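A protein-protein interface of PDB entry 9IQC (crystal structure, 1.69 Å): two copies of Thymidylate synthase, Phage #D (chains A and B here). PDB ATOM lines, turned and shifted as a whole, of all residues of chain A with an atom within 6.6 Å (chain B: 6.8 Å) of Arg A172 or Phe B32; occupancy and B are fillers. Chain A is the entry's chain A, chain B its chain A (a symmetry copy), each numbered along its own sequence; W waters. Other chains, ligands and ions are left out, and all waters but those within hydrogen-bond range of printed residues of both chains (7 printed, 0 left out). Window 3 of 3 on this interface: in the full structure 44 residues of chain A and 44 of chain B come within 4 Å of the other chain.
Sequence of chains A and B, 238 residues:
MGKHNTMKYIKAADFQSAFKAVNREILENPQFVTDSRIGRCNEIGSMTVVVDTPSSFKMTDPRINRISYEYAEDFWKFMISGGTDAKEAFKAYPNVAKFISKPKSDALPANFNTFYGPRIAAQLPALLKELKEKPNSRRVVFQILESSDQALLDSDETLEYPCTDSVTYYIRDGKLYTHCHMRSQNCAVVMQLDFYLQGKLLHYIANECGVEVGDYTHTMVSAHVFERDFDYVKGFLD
NH1 of Arg A138 lies close to OG of Ser B36 (3.3 Å). NE of Arg A172 is in salt-bridge range of OE1 of Glu B43 (2.7 Å).
NH1 of Arg A172 sits close to O of Asn A136 (3.4 Å). The backbone carbonyl oxygen of Ser A137 sits at hydrogen-bond distance from the guanidinium group of Arg A172. O of Tyr A170 lies within hydrogen-bond range of N of Tyr A177 (2.7 Å). The side-chain amino group (NZ) of Lys B8 lies within hydrogen-bond range of the side-chain amide oxygen (OE1) of Gln B31 (2.8 Å). The side-chain amino group (NZ) of Lys B8 is in hydrogen-bond range of the backbone carbonyl oxygen (O) of Gly B45. O of Thr B34 is in hydrogen-bond range of N of Cys B41 (2.9 Å).
Among the printed residues, merely in contact across the chains: Asn A136 with Thr B34 (3.2 Å), Arg A138 with Ser B222 (3.3 Å), Tyr A170 with Gly B45 (3.4 Å), Arg A172 with Phe B32 (3.5 Å), Tyr A177 with Phe B32 (3.7 Å), Tyr A170 with Phe B32 (3.7 Å), Arg A172 with Thr B34 (3.8 Å), Tyr A170 with Val B221 (3.8 Å), Tyr A177 with Gln B31 (3.9 Å) and Arg A138 with Cys B41 (3.9 Å).
Of the printed residues of chain B, Arg A138 touches Ser B36, Cys B41 and Ser B222. Of chain B, only Phe B32, Thr B34 and Glu B43 come within 4 Å of Arg A172. Printed residues of chain A within 4 Å of Gln B31: Tyr A177. The nearest residue of chain B that does not touch Arg A172 is Ser B222 (4.7 Å).
Of the 13 printed residues of chain A, 5 touch a printed residue of chain B. Printed residues of chain A that touch a printed residue of chain B: Asn A136, Arg A138, Tyr A170, Arg A172 and Tyr A177. Along chain A the printed residues that touch a printed residue of chain B span positions 136 to 177. Of the 17 printed residues of chain B, 9 touch a printed residue of chain A. Printed residues of chain B that touch a printed residue of chain A: Gln B31, Phe B32, Thr B34, Ser B36, Cys B41, Glu B43, Gly B45, Val B221 and Ser B222. Hydrophobic or aromatic side chains of chain B within 4 Å of the printed part of chain A: Phe B32 and Val B221. Among the printed residues, 12 pairs touch across the chains. Among the printed residues, Asp or Glu carboxylates within 4 Å of a Lys or Arg side-chain nitrogen of the other chain: Arg A172 with Glu B43 (2.7 Å).
No position is printed for both chains.
Water W1 lies within hydrogen-bond range of the backbone carbonyl oxygen of Pro A135 (2.6 Å) and the backbone carbonyl oxygen of Ser B36 (3.4 Å). Water W5 lies within hydrogen-bond range of the side-chain hydroxyl of Thr B34 and the side-chain amide nitrogen of Asn A136. Water W6 bridges OD2 of Asp A173 (2.8 Å) and O of Val B33 (3.1 Å). Water W3 bridges O of Asn A136 (2.8 Å) and OG1 of Thr B34 (3.3 Å). Water W7 bridges N of Val B33 (2.8 Å) and OD2 of Asp A173 (3.5 Å). Water W2 lies within hydrogen-bond range of OH of Tyr A177 and NE2 of Gln B31.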
ATOM      1  N   PRO A 135     -25.524  18.728   1.120  1.00  0.00           N
ATOM      2  CA  PRO A 135     -25.999  18.516  -0.255  1.00  0.00           C
ATOM      3  C   PRO A 135     -24.861  18.631  -1.256  1.00  0.00           C
ATOM      4  O   PRO A 135     -24.065  19.568  -1.205  1.00  0.00           O
ATOM      5  CB  PRO A 135     -27.029  19.636  -0.452  1.00  0.00           C
ATOM      6  CG  PRO A 135     -27.440  20.023   0.924  1.00  0.00           C
ATOM      7  CD  PRO A 135     -26.236  19.829   1.790  1.00  0.00           C
ATOM      8  N   ASN A 136     -24.792  17.658  -2.168  1.00  0.00           N
ATOM      9  CA  ASN A 136     -23.832  17.673  -3.279  1.00  0.00           C
ATOM     10  C   ASN A 136     -22.394  17.731  -2.789  1.00  0.00           C
ATOM     11  O   ASN A 136     -21.516  18.294  -3.460  1.00  0.00           O
ATOM     12  CB  ASN A 136     -24.127  18.822  -4.240  1.00  0.00           C
ATOM     13  CG  ASN A 136     -25.588  18.854  -4.657  1.00  0.00           C
ATOM     14  OD1 ASN A 136     -26.275  19.864  -4.495  1.00  0.00           O
ATOM     15  ND2 ASN A 136     -26.071  17.737  -5.180  1.00  0.00           N
ATOM     16  N   SER A 137     -22.142  17.129  -1.627  1.00  0.00           N
ATOM     17  CA  SER A 137     -20.790  17.074  -1.091  1.00  0.00           C
ATOM     18  C   SER A 137     -19.837  16.402  -2.071  1.00  0.00           C
ATOM     19  O   SER A 137     -20.204  15.462  -2.786  1.00  0.00           O
ATOM     20  CB  SER A 137     -20.779  16.312   0.231  1.00  0.00           C
ATOM     21  OG  SER A 137     -19.450  16.099   0.667  1.00  0.00           O
ATOM     22  N   ARG A 138     -18.602  16.897  -2.099  1.00  0.00           N
ATOM     23  CA  ARG A 138     -17.505  16.236  -2.789  1.00  0.00           C
ATOM     24  C   ARG A 138     -16.572  15.536  -1.821  1.00  0.00           C
ATOM     25  O   ARG A 138     -15.496  15.082  -2.229  1.00  0.00           O
ATOM     26  CB  ARG A 138     -16.705  17.253  -3.611  1.00  0.00           C
ATOM     27  CG  ARG A 138     -17.496  17.920  -4.704  1.00  0.00           C
ATOM     28  CD  ARG A 138     -16.666  19.068  -5.299  1.00  0.00           C
ATOM     29  NE  ARG A 138     -16.567  20.187  -4.369  1.00  0.00           N
ATOM     30  CZ  ARG A 138     -17.086  21.391  -4.578  1.00  0.00           C
ATOM     31  NH1 ARG A 138     -17.740  21.679  -5.693  1.00  0.00           N
ATOM     32  NH2 ARG A 138     -16.929  22.335  -3.653  1.00  0.00           N
ATOM     33  N   TYR A 169     -17.717   8.430  -2.799  1.00  0.00           N
ATOM     34  CA  TYR A 169     -19.138   8.401  -3.095  1.00  0.00           C
ATOM     35  C   TYR A 169     -19.638   9.824  -3.199  1.00  0.00           C
ATOM     36  O   TYR A 169     -19.254  10.684  -2.398  1.00  0.00           O
ATOM     37  CB  TYR A 169     -19.927   7.679  -2.001  1.00  0.00           C
ATOM     38  CG  TYR A 169     -19.604   6.221  -1.892  1.00  0.00           C
ATOM     39  CD1 TYR A 169     -19.978   5.341  -2.894  1.00  0.00           C
ATOM     40  CD2 TYR A 169     -18.906   5.723  -0.797  1.00  0.00           C
ATOM     41  CE1 TYR A 169     -19.676   3.996  -2.806  1.00  0.00           C
ATOM     42  CE2 TYR A 169     -18.598   4.382  -0.697  1.00  0.00           C
ATOM     43  CZ  TYR A 169     -18.995   3.523  -1.703  1.00  0.00           C
ATOM     44  OH  TYR A 169     -18.687   2.185  -1.625  1.00  0.00           O
ATOM     45  N   TYR A 170     -20.526  10.066  -4.156  1.00  0.00           N
ATOM     46  CA  TYR A 170     -21.179  11.360  -4.182  1.00  0.00           C
ATOM     47  C   TYR A 170     -22.561  11.186  -4.782  1.00  0.00           C
ATOM     48  O   TYR A 170     -22.815  10.245  -5.541  1.00  0.00           O
ATOM     49  CB  TYR A 170     -20.340  12.409  -4.941  1.00  0.00           C
ATOM     50  CG  TYR A 170     -20.159  12.140  -6.414  1.00  0.00           C
ATOM     51  CD1 TYR A 170     -19.089  11.374  -6.880  1.00  0.00           C
ATOM     52  CD2 TYR A 170     -21.046  12.664  -7.338  1.00  0.00           C
ATOM     53  CE1 TYR A 170     -18.917  11.137  -8.238  1.00  0.00           C
ATOM     54  CE2 TYR A 170     -20.890  12.435  -8.692  1.00  0.00           C
ATOM     55  CZ  TYR A 170     -19.830  11.675  -9.135  1.00  0.00           C
ATOM     56  OH  TYR A 170     -19.704  11.441 -10.474  1.00  0.00           O
ATOM     57  N   ILE A 171     -23.460  12.085  -4.404  1.00  0.00           N
ATOM     58  CA  ILE A 171     -24.859  12.008  -4.794  1.00  0.00           C
ATOM     59  C   ILE A 171     -25.202  13.272  -5.563  1.00  0.00           C
ATOM     60  O   ILE A 171     -24.938  14.380  -5.089  1.00  0.00           O
ATOM     61  CB  ILE A 171     -25.772  11.836  -3.567  1.00  0.00           C
ATOM     62  CG1 ILE A 171     -25.564  10.436  -2.961  1.00  0.00           C
ATOM     63  CG2 ILE A 171     -27.222  12.039  -3.971  1.00  0.00           C
ATOM     64  CD1 ILE A 171     -26.194  10.236  -1.609  1.00  0.00           C
ATOM     65  N   ARG A 172     -25.760  13.102  -6.758  1.00  0.00           N
ATOM     66  CA  ARG A 172     -26.251  14.206  -7.572  1.00  0.00           C
ATOM     67  C   ARG A 172     -27.624  13.817  -8.091  1.00  0.00           C
ATOM     68  O   ARG A 172     -27.773  12.744  -8.681  1.00  0.00           O
ATOM     69  CB  ARG A 172     -25.358  14.498  -8.768  1.00  0.00           C
ATOM     70  CG  ARG A 172     -23.880  14.806  -8.463  1.00  0.00           C
ATOM     71  CD  ARG A 172     -23.711  16.115  -7.693  1.00  0.00           C
ATOM     72  NE  ARG A 172     -22.292  16.412  -7.481  1.00  0.00           N
ATOM     73  CZ  ARG A 172     -21.625  16.122  -6.368  1.00  0.00           C
ATOM     74  NH1 ARG A 172     -22.222  15.577  -5.324  1.00  0.00           N
ATOM     75  NH2 ARG A 172     -20.325  16.383  -6.302  1.00  0.00           N
ATOM     76  N   ASP A 173     -28.605  14.691  -7.897  1.00  0.00           N
ATOM     77  CA  ASP A 173     -29.928  14.509  -8.495  1.00  0.00           C
ATOM     78  C   ASP A 173     -30.479  13.118  -8.192  1.00  0.00           C
ATOM     79  O   ASP A 173     -30.948  12.402  -9.079  1.00  0.00           O
ATOM     80  CB  ASP A 173     -29.878  14.747 -10.007  1.00  0.00           C
ATOM     81  CG  ASP A 173     -29.357  16.128 -10.371  1.00  0.00           C
ATOM     82  OD1 ASP A 173     -29.685  17.102  -9.666  1.00  0.00           O
ATOM     83  OD2 ASP A 173     -28.630  16.230 -11.375  1.00  0.00           O
ATOM     84  N   GLY A 174     -30.377  12.717  -6.929  1.00  0.00           N
ATOM     85  CA  GLY A 174     -31.009  11.497  -6.459  1.00  0.00           C
ATOM     86  C   GLY A 174     -30.258  10.214  -6.738  1.00  0.00           C
ATOM     87  O   GLY A 174     -30.794   9.140  -6.456  1.00  0.00           O
ATOM     88  N   LYS A 175     -29.029  10.279  -7.265  1.00  0.00           N
ATOM     89  CA  LYS A 175     -28.293   9.078  -7.640  1.00  0.00           C
ATOM     90  C   LYS A 175     -26.907   9.067  -7.007  1.00  0.00           C
ATOM     91  O   LYS A 175     -26.224  10.095  -6.964  1.00  0.00           O
ATOM     92  CB  LYS A 175     -28.164   8.954  -9.165  1.00  0.00           C
ATOM     93  CG  LYS A 175     -29.474   8.543  -9.857  1.00  0.00           C
ATOM     94  CD  LYS A 175     -29.297   8.485 -11.366  1.00  0.00           C
ATOM     95  CE  LYS A 175     -30.451   7.742 -12.007  1.00  0.00           C
ATOM     96  NZ  LYS A 175     -31.708   8.067 -11.273  1.00  0.00           N
ATOM     97  N   LEU A 176     -26.511   7.889  -6.514  1.00  0.00           N
ATOM     98  CA  LEU A 176     -25.193   7.667  -5.925  1.00  0.00           C
ATOM     99  C   LEU A 176     -24.179   7.293  -7.000  1.00  0.00           C
ATOM    100  O   LEU A 176     -24.367   6.311  -7.727  1.00  0.00           O
ATOM    101  CB  LEU A 176     -25.263   6.554  -4.882  1.00  0.00           C
ATOM    102  CG  LEU A 176     -23.901   6.202  -4.281  1.00  0.00           C
ATOM    103  CD1 LEU A 176     -23.464   7.262  -3.289  1.00  0.00           C
ATOM    104  CD2 LEU A 176     -23.959   4.823  -3.629  1.00  0.00           C
ATOM    105  N   TYR A 177     -23.090   8.056  -7.079  1.00  0.00           N
ATOM    106  CA  TYR A 177     -21.986   7.778  -7.984  1.00  0.00           C
ATOM    107  C   TYR A 177     -20.790   7.323  -7.165  1.00  0.00           C
ATOM    108  O   TYR A 177     -20.583   7.789  -6.043  1.00  0.00           O
ATOM    109  CB  TYR A 177     -21.631   9.008  -8.823  1.00  0.00           C
ATOM    110  CG  TYR A 177     -22.762   9.393  -9.738  1.00  0.00           C
ATOM    111  CD1 TYR A 177     -23.813  10.180  -9.275  1.00  0.00           C
ATOM    112  CD2 TYR A 177     -22.811   8.928 -11.046  1.00  0.00           C
ATOM    113  CE1 TYR A 177     -24.883  10.502 -10.097  1.00  0.00           C
ATOM    114  CE2 TYR A 177     -23.870   9.249 -11.876  1.00  0.00           C
ATOM    115  CZ  TYR A 177     -24.901  10.036 -11.394  1.00  0.00           C
ATOM    116  OH  TYR A 177     -25.962  10.362 -12.208  1.00  0.00           O
ATOM    117  N   THR B   6     -20.497  14.105 -23.054  1.00  0.00           N
ATOM    118  CA  THR B   6     -19.465  14.504 -22.104  1.00  0.00           C
ATOM    119  C   THR B   6     -18.218  13.654 -22.284  1.00  0.00           C
ATOM    120  O   THR B   6     -18.276  12.423 -22.186  1.00  0.00           O
ATOM    121  CB  THR B   6     -19.993  14.378 -20.676  1.00  0.00           C
ATOM    122  OG1 THR B   6     -21.043  15.330 -20.479  1.00  0.00           O
ATOM    123  CG2 THR B   6     -18.891  14.647 -19.678  1.00  0.00           C
ATOM    124  N   LYS B   8     -14.877  12.382 -20.877  1.00  0.00           N
ATOM    125  CA  LYS B   8     -14.274  12.209 -19.563  1.00  0.00           C
ATOM    126  C   LYS B   8     -12.812  11.814 -19.612  1.00  0.00           C
ATOM    127  O   LYS B   8     -12.162  11.786 -18.561  1.00  0.00           O
ATOM    128  CB  LYS B   8     -15.028  11.148 -18.766  1.00  0.00           C
ATOM    129  CG  LYS B   8     -16.415  11.556 -18.425  1.00  0.00           C
ATOM    130  CD  LYS B   8     -16.948  10.658 -17.342  1.00  0.00           C
ATOM    131  CE  LYS B   8     -18.272  11.167 -16.845  1.00  0.00           C
ATOM    132  NZ  LYS B   8     -18.570  10.559 -15.534  1.00  0.00           N
ATOM    133  N   ILE B  26     -15.836  20.997 -19.311  1.00  0.00           N
ATOM    134  CA  ILE B  26     -16.709  21.245 -18.167  1.00  0.00           C
ATOM    135  C   ILE B  26     -17.686  22.371 -18.481  1.00  0.00           C
ATOM    136  O   ILE B  26     -18.862  22.316 -18.104  1.00  0.00           O
ATOM    137  CB  ILE B  26     -15.870  21.551 -16.915  1.00  0.00           C
ATOM    138  CG1 ILE B  26     -15.043  20.330 -16.517  1.00  0.00           C
ATOM    139  CG2 ILE B  26     -16.764  21.999 -15.761  1.00  0.00           C
ATOM    140  CD1 ILE B  26     -14.029  20.632 -15.434  1.00  0.00           C
ATOM    141  N   ASN B  29     -19.923  20.740 -21.877  1.00  0.00           N
ATOM    142  CA  ASN B  29     -20.608  19.445 -21.775  1.00  0.00           C
ATOM    143  C   ASN B  29     -20.582  18.906 -20.349  1.00  0.00           C
ATOM    144  O   ASN B  29     -20.082  17.802 -20.104  1.00  0.00           O
ATOM    145  CB  ASN B  29     -19.977  18.433 -22.729  1.00  0.00           C
ATOM    146  CG  ASN B  29     -20.041  18.867 -24.172  1.00  0.00           C
ATOM    147  OD1 ASN B  29     -21.078  19.334 -24.647  1.00  0.00           O
ATOM    148  ND2 ASN B  29     -18.925  18.721 -24.883  1.00  0.00           N
ATOM    149  N   PRO B  30     -21.122  19.644 -19.381  1.00  0.00           N
ATOM    150  CA  PRO B  30     -21.064  19.169 -17.996  1.00  0.00           C
ATOM    151  C   PRO B  30     -21.886  17.905 -17.824  1.00  0.00           C
ATOM    152  O   PRO B  30     -22.880  17.686 -18.515  1.00  0.00           O
ATOM    153  CB  PRO B  30     -21.663  20.327 -17.191  1.00  0.00           C
ATOM    154  CG  PRO B  30     -22.607  20.987 -18.161  1.00  0.00           C
ATOM    155  CD  PRO B  30     -21.886  20.904 -19.486  1.00  0.00           C
ATOM    156  N   GLN B  31     -21.440  17.056 -16.902  1.00  0.00           N
ATOM    157  CA  GLN B  31     -22.292  15.956 -16.466  1.00  0.00           C
ATOM    158  C   GLN B  31     -23.354  16.449 -15.495  1.00  0.00           C
ATOM    159  O   GLN B  31     -24.513  16.011 -15.546  1.00  0.00           O
ATOM    160  CB  GLN B  31     -21.442  14.863 -15.819  1.00  0.00           C
ATOM    161  CG  GLN B  31     -22.251  13.666 -15.303  1.00  0.00           C
ATOM    162  CD  GLN B  31     -21.354  12.550 -14.795  1.00  0.00           C
ATOM    163  OE1 GLN B  31     -20.130  12.714 -14.698  1.00  0.00           O
ATOM    164  NE2 GLN B  31     -21.948  11.410 -14.474  1.00  0.00           N
ATOM    165  N   PHE B  32     -22.979  17.367 -14.612  1.00  0.00           N
ATOM    166  CA  PHE B  32     -23.875  17.920 -13.616  1.00  0.00           C
ATOM    167  C   PHE B  32     -23.751  19.433 -13.613  1.00  0.00           C
ATOM    168  O   PHE B  32     -22.676  19.983 -13.847  1.00  0.00           O
ATOM    169  CB  PHE B  32     -23.560  17.412 -12.205  1.00  0.00           C
ATOM    170  CG  PHE B  32     -23.386  15.924 -12.113  1.00  0.00           C
ATOM    171  CD1 PHE B  32     -24.494  15.075 -12.137  1.00  0.00           C
ATOM    172  CD2 PHE B  32     -22.124  15.371 -11.937  1.00  0.00           C
ATOM    173  CE1 PHE B  32     -24.328  13.700 -12.034  1.00  0.00           C
ATOM    174  CE2 PHE B  32     -21.953  14.000 -11.829  1.00  0.00           C
ATOM    175  CZ  PHE B  32     -23.059  13.163 -11.877  1.00  0.00           C
ATOM    176  N   VAL B  33     -24.865  20.097 -13.347  1.00  0.00           N
ATOM    177  CA  VAL B  33     -24.862  21.501 -12.963  1.00  0.00           C
ATOM    178  C   VAL B  33     -25.397  21.515 -11.541  1.00  0.00           C
ATOM    179  O   VAL B  33     -26.563  21.164 -11.304  1.00  0.00           O
ATOM    180  CB  VAL B  33     -25.696  22.372 -13.910  1.00  0.00           C
ATOM    181  CG1 VAL B  33     -25.725  23.805 -13.414  1.00  0.00           C
ATOM    182  CG2 VAL B  33     -25.133  22.307 -15.315  1.00  0.00           C
ATOM    183  N   THR B  34     -24.540  21.854 -10.586  1.00  0.00           N
ATOM    184  CA  THR B  34     -24.811  21.498  -9.202  1.00  0.00           C
ATOM    185  C   THR B  34     -24.458  22.630  -8.249  1.00  0.00           C
ATOM    186  O   THR B  34     -23.469  23.345  -8.438  1.00  0.00           O
ATOM    187  CB  THR B  34     -24.053  20.213  -8.816  1.00  0.00           C
ATOM    188  OG1 THR B  34     -24.367  19.848  -7.467  1.00  0.00           O
ATOM    189  CG2 THR B  34     -22.552  20.393  -8.960  1.00  0.00           C
ATOM    190  N   SER B  36     -22.936  23.459  -4.978  1.00  0.00           N
ATOM    191  CA  SER B  36     -21.959  22.800  -4.133  1.00  0.00           C
ATOM    192  C   SER B  36     -21.807  23.526  -2.802  1.00  0.00           C
ATOM    193  O   SER B  36     -22.410  24.573  -2.549  1.00  0.00           O
ATOM    194  CB  SER B  36     -20.611  22.716  -4.846  1.00  0.00           C
ATOM    195  OG  SER B  36     -19.883  23.923  -4.667  1.00  0.00           O
ATOM    196  N   CYS B  41     -21.679  25.179  -9.744  1.00  0.00           N
ATOM    197  CA  CYS B  41     -20.605  24.842 -10.667  1.00  0.00           C
ATOM    198  C   CYS B  41     -21.090  23.839 -11.703  1.00  0.00           C
ATOM    199  O   CYS B  41     -22.028  23.070 -11.460  1.00  0.00           O
ATOM    200  CB  CYS B  41     -19.392  24.282  -9.919  1.00  0.00           C
ATOM    201  SG  CYS B  41     -19.729  22.823  -8.905  1.00  0.00           S
ATOM    202  N   ASN B  42     -20.462  23.887 -12.876  1.00  0.00           N
ATOM    203  CA  ASN B  42     -20.514  22.779 -13.814  1.00  0.00           C
ATOM    204  C   ASN B  42     -19.522  21.726 -13.360  1.00  0.00           C
ATOM    205  O   ASN B  42     -18.427  22.052 -12.890  1.00  0.00           O
ATOM    206  CB  ASN B  42     -20.161  23.227 -15.234  1.00  0.00           C
ATOM    207  CG  ASN B  42     -21.304  23.929 -15.930  1.00  0.00           C
ATOM    208  OD1 ASN B  42     -22.255  24.387 -15.287  1.00  0.00           O
ATOM    209  ND2 ASN B  42     -21.224  24.009 -17.250  1.00  0.00           N
ATOM    210  N   GLU B  43     -19.889  20.465 -13.531  1.00  0.00           N
ATOM    211  CA  GLU B  43     -19.087  19.393 -12.972  1.00  0.00           C
ATOM    212  C   GLU B  43     -19.084  18.201 -13.913  1.00  0.00           C
ATOM    213  O   GLU B  43     -20.096  17.889 -14.543  1.00  0.00           O
ATOM    214  CB  GLU B  43     -19.632  19.002 -11.592  1.00  0.00           C
ATOM    215  CG  GLU B  43     -18.939  17.850 -10.896  1.00  0.00           C
ATOM    216  CD  GLU B  43     -19.591  17.546  -9.564  1.00  0.00           C
ATOM    217  OE1 GLU B  43     -20.808  17.267  -9.560  1.00  0.00           O
ATOM    218  OE2 GLU B  43     -18.912  17.622  -8.517  1.00  0.00           O
ATOM    219  N   ILE B  44     -17.938  17.537 -14.011  1.00  0.00           N
ATOM    220  CA  ILE B  44     -17.863  16.235 -14.654  1.00  0.00           C
ATOM    221  C   ILE B  44     -17.276  15.270 -13.640  1.00  0.00           C
ATOM    222  O   ILE B  44     -16.223  15.544 -13.050  1.00  0.00           O
ATOM    223  CB  ILE B  44     -17.033  16.272 -15.950  1.00  0.00           C
ATOM    224  CG1 ILE B  44     -17.708  17.167 -16.998  1.00  0.00           C
ATOM    225  CG2 ILE B  44     -16.882  14.866 -16.526  1.00  0.00           C
ATOM    226  CD1 ILE B  44     -16.818  17.429 -18.232  1.00  0.00           C
ATOM    227  N   GLY B  45     -17.974  14.162 -13.411  1.00  0.00           N
ATOM    228  CA  GLY B  45     -17.492  13.182 -12.467  1.00  0.00           C
ATOM    229  C   GLY B  45     -16.450  12.278 -13.103  1.00  0.00           C
ATOM    230  O   GLY B  45     -16.553  11.896 -14.268  1.00  0.00           O
ATOM    231  N   VAL B 221     -12.326  12.956  -9.134  1.00  0.00           N
ATOM    232  CA  VAL B 221     -13.667  12.437  -8.893  1.00  0.00           C
ATOM    233  C   VAL B 221     -14.704  13.516  -9.185  1.00  0.00           C
ATOM    234  O   VAL B 221     -15.731  13.263  -9.826  1.00  0.00           O
ATOM    235  CB  VAL B 221     -13.804  11.892  -7.466  1.00  0.00           C
ATOM    236  CG1 VAL B 221     -15.232  11.336  -7.289  1.00  0.00           C
ATOM    237  CG2 VAL B 221     -12.805  10.776  -7.229  1.00  0.00           C
ATOM    238  N   SER B 222     -14.454  14.731  -8.712  1.00  0.00           N
ATOM    239  CA  SER B 222     -15.206  15.908  -9.130  1.00  0.00           C
ATOM    240  C   SER B 222     -14.268  16.853  -9.861  1.00  0.00           C
ATOM    241  O   SER B 222     -13.340  17.387  -9.255  1.00  0.00           O
ATOM    242  CB  SER B 222     -15.825  16.633  -7.943  1.00  0.00           C
ATOM    243  OG  SER B 222     -16.393  17.849  -8.387  1.00  0.00           O
HETATM  244  O   HOH W   1     -24.580  22.046  -1.747  1.00  0.00           O
HETATM  245  O   HOH W   2     -24.928  11.280 -14.764  1.00  0.00           O
HETATM  246  O   HOH W   3     -21.469  19.835  -5.841  1.00  0.00           O
HETATM  247  O   HOH W   4     -19.335  20.041  -7.322  1.00  0.00           O
HETATM  248  O   HOH W   5     -26.852  18.892  -7.723  1.00  0.00           O
HETATM  249  O   HOH W   6     -26.810  18.173 -10.505  1.00  0.00           O
HETATM  250  O   HOH W   7     -27.339  18.692 -13.496  1.00  0.00           O
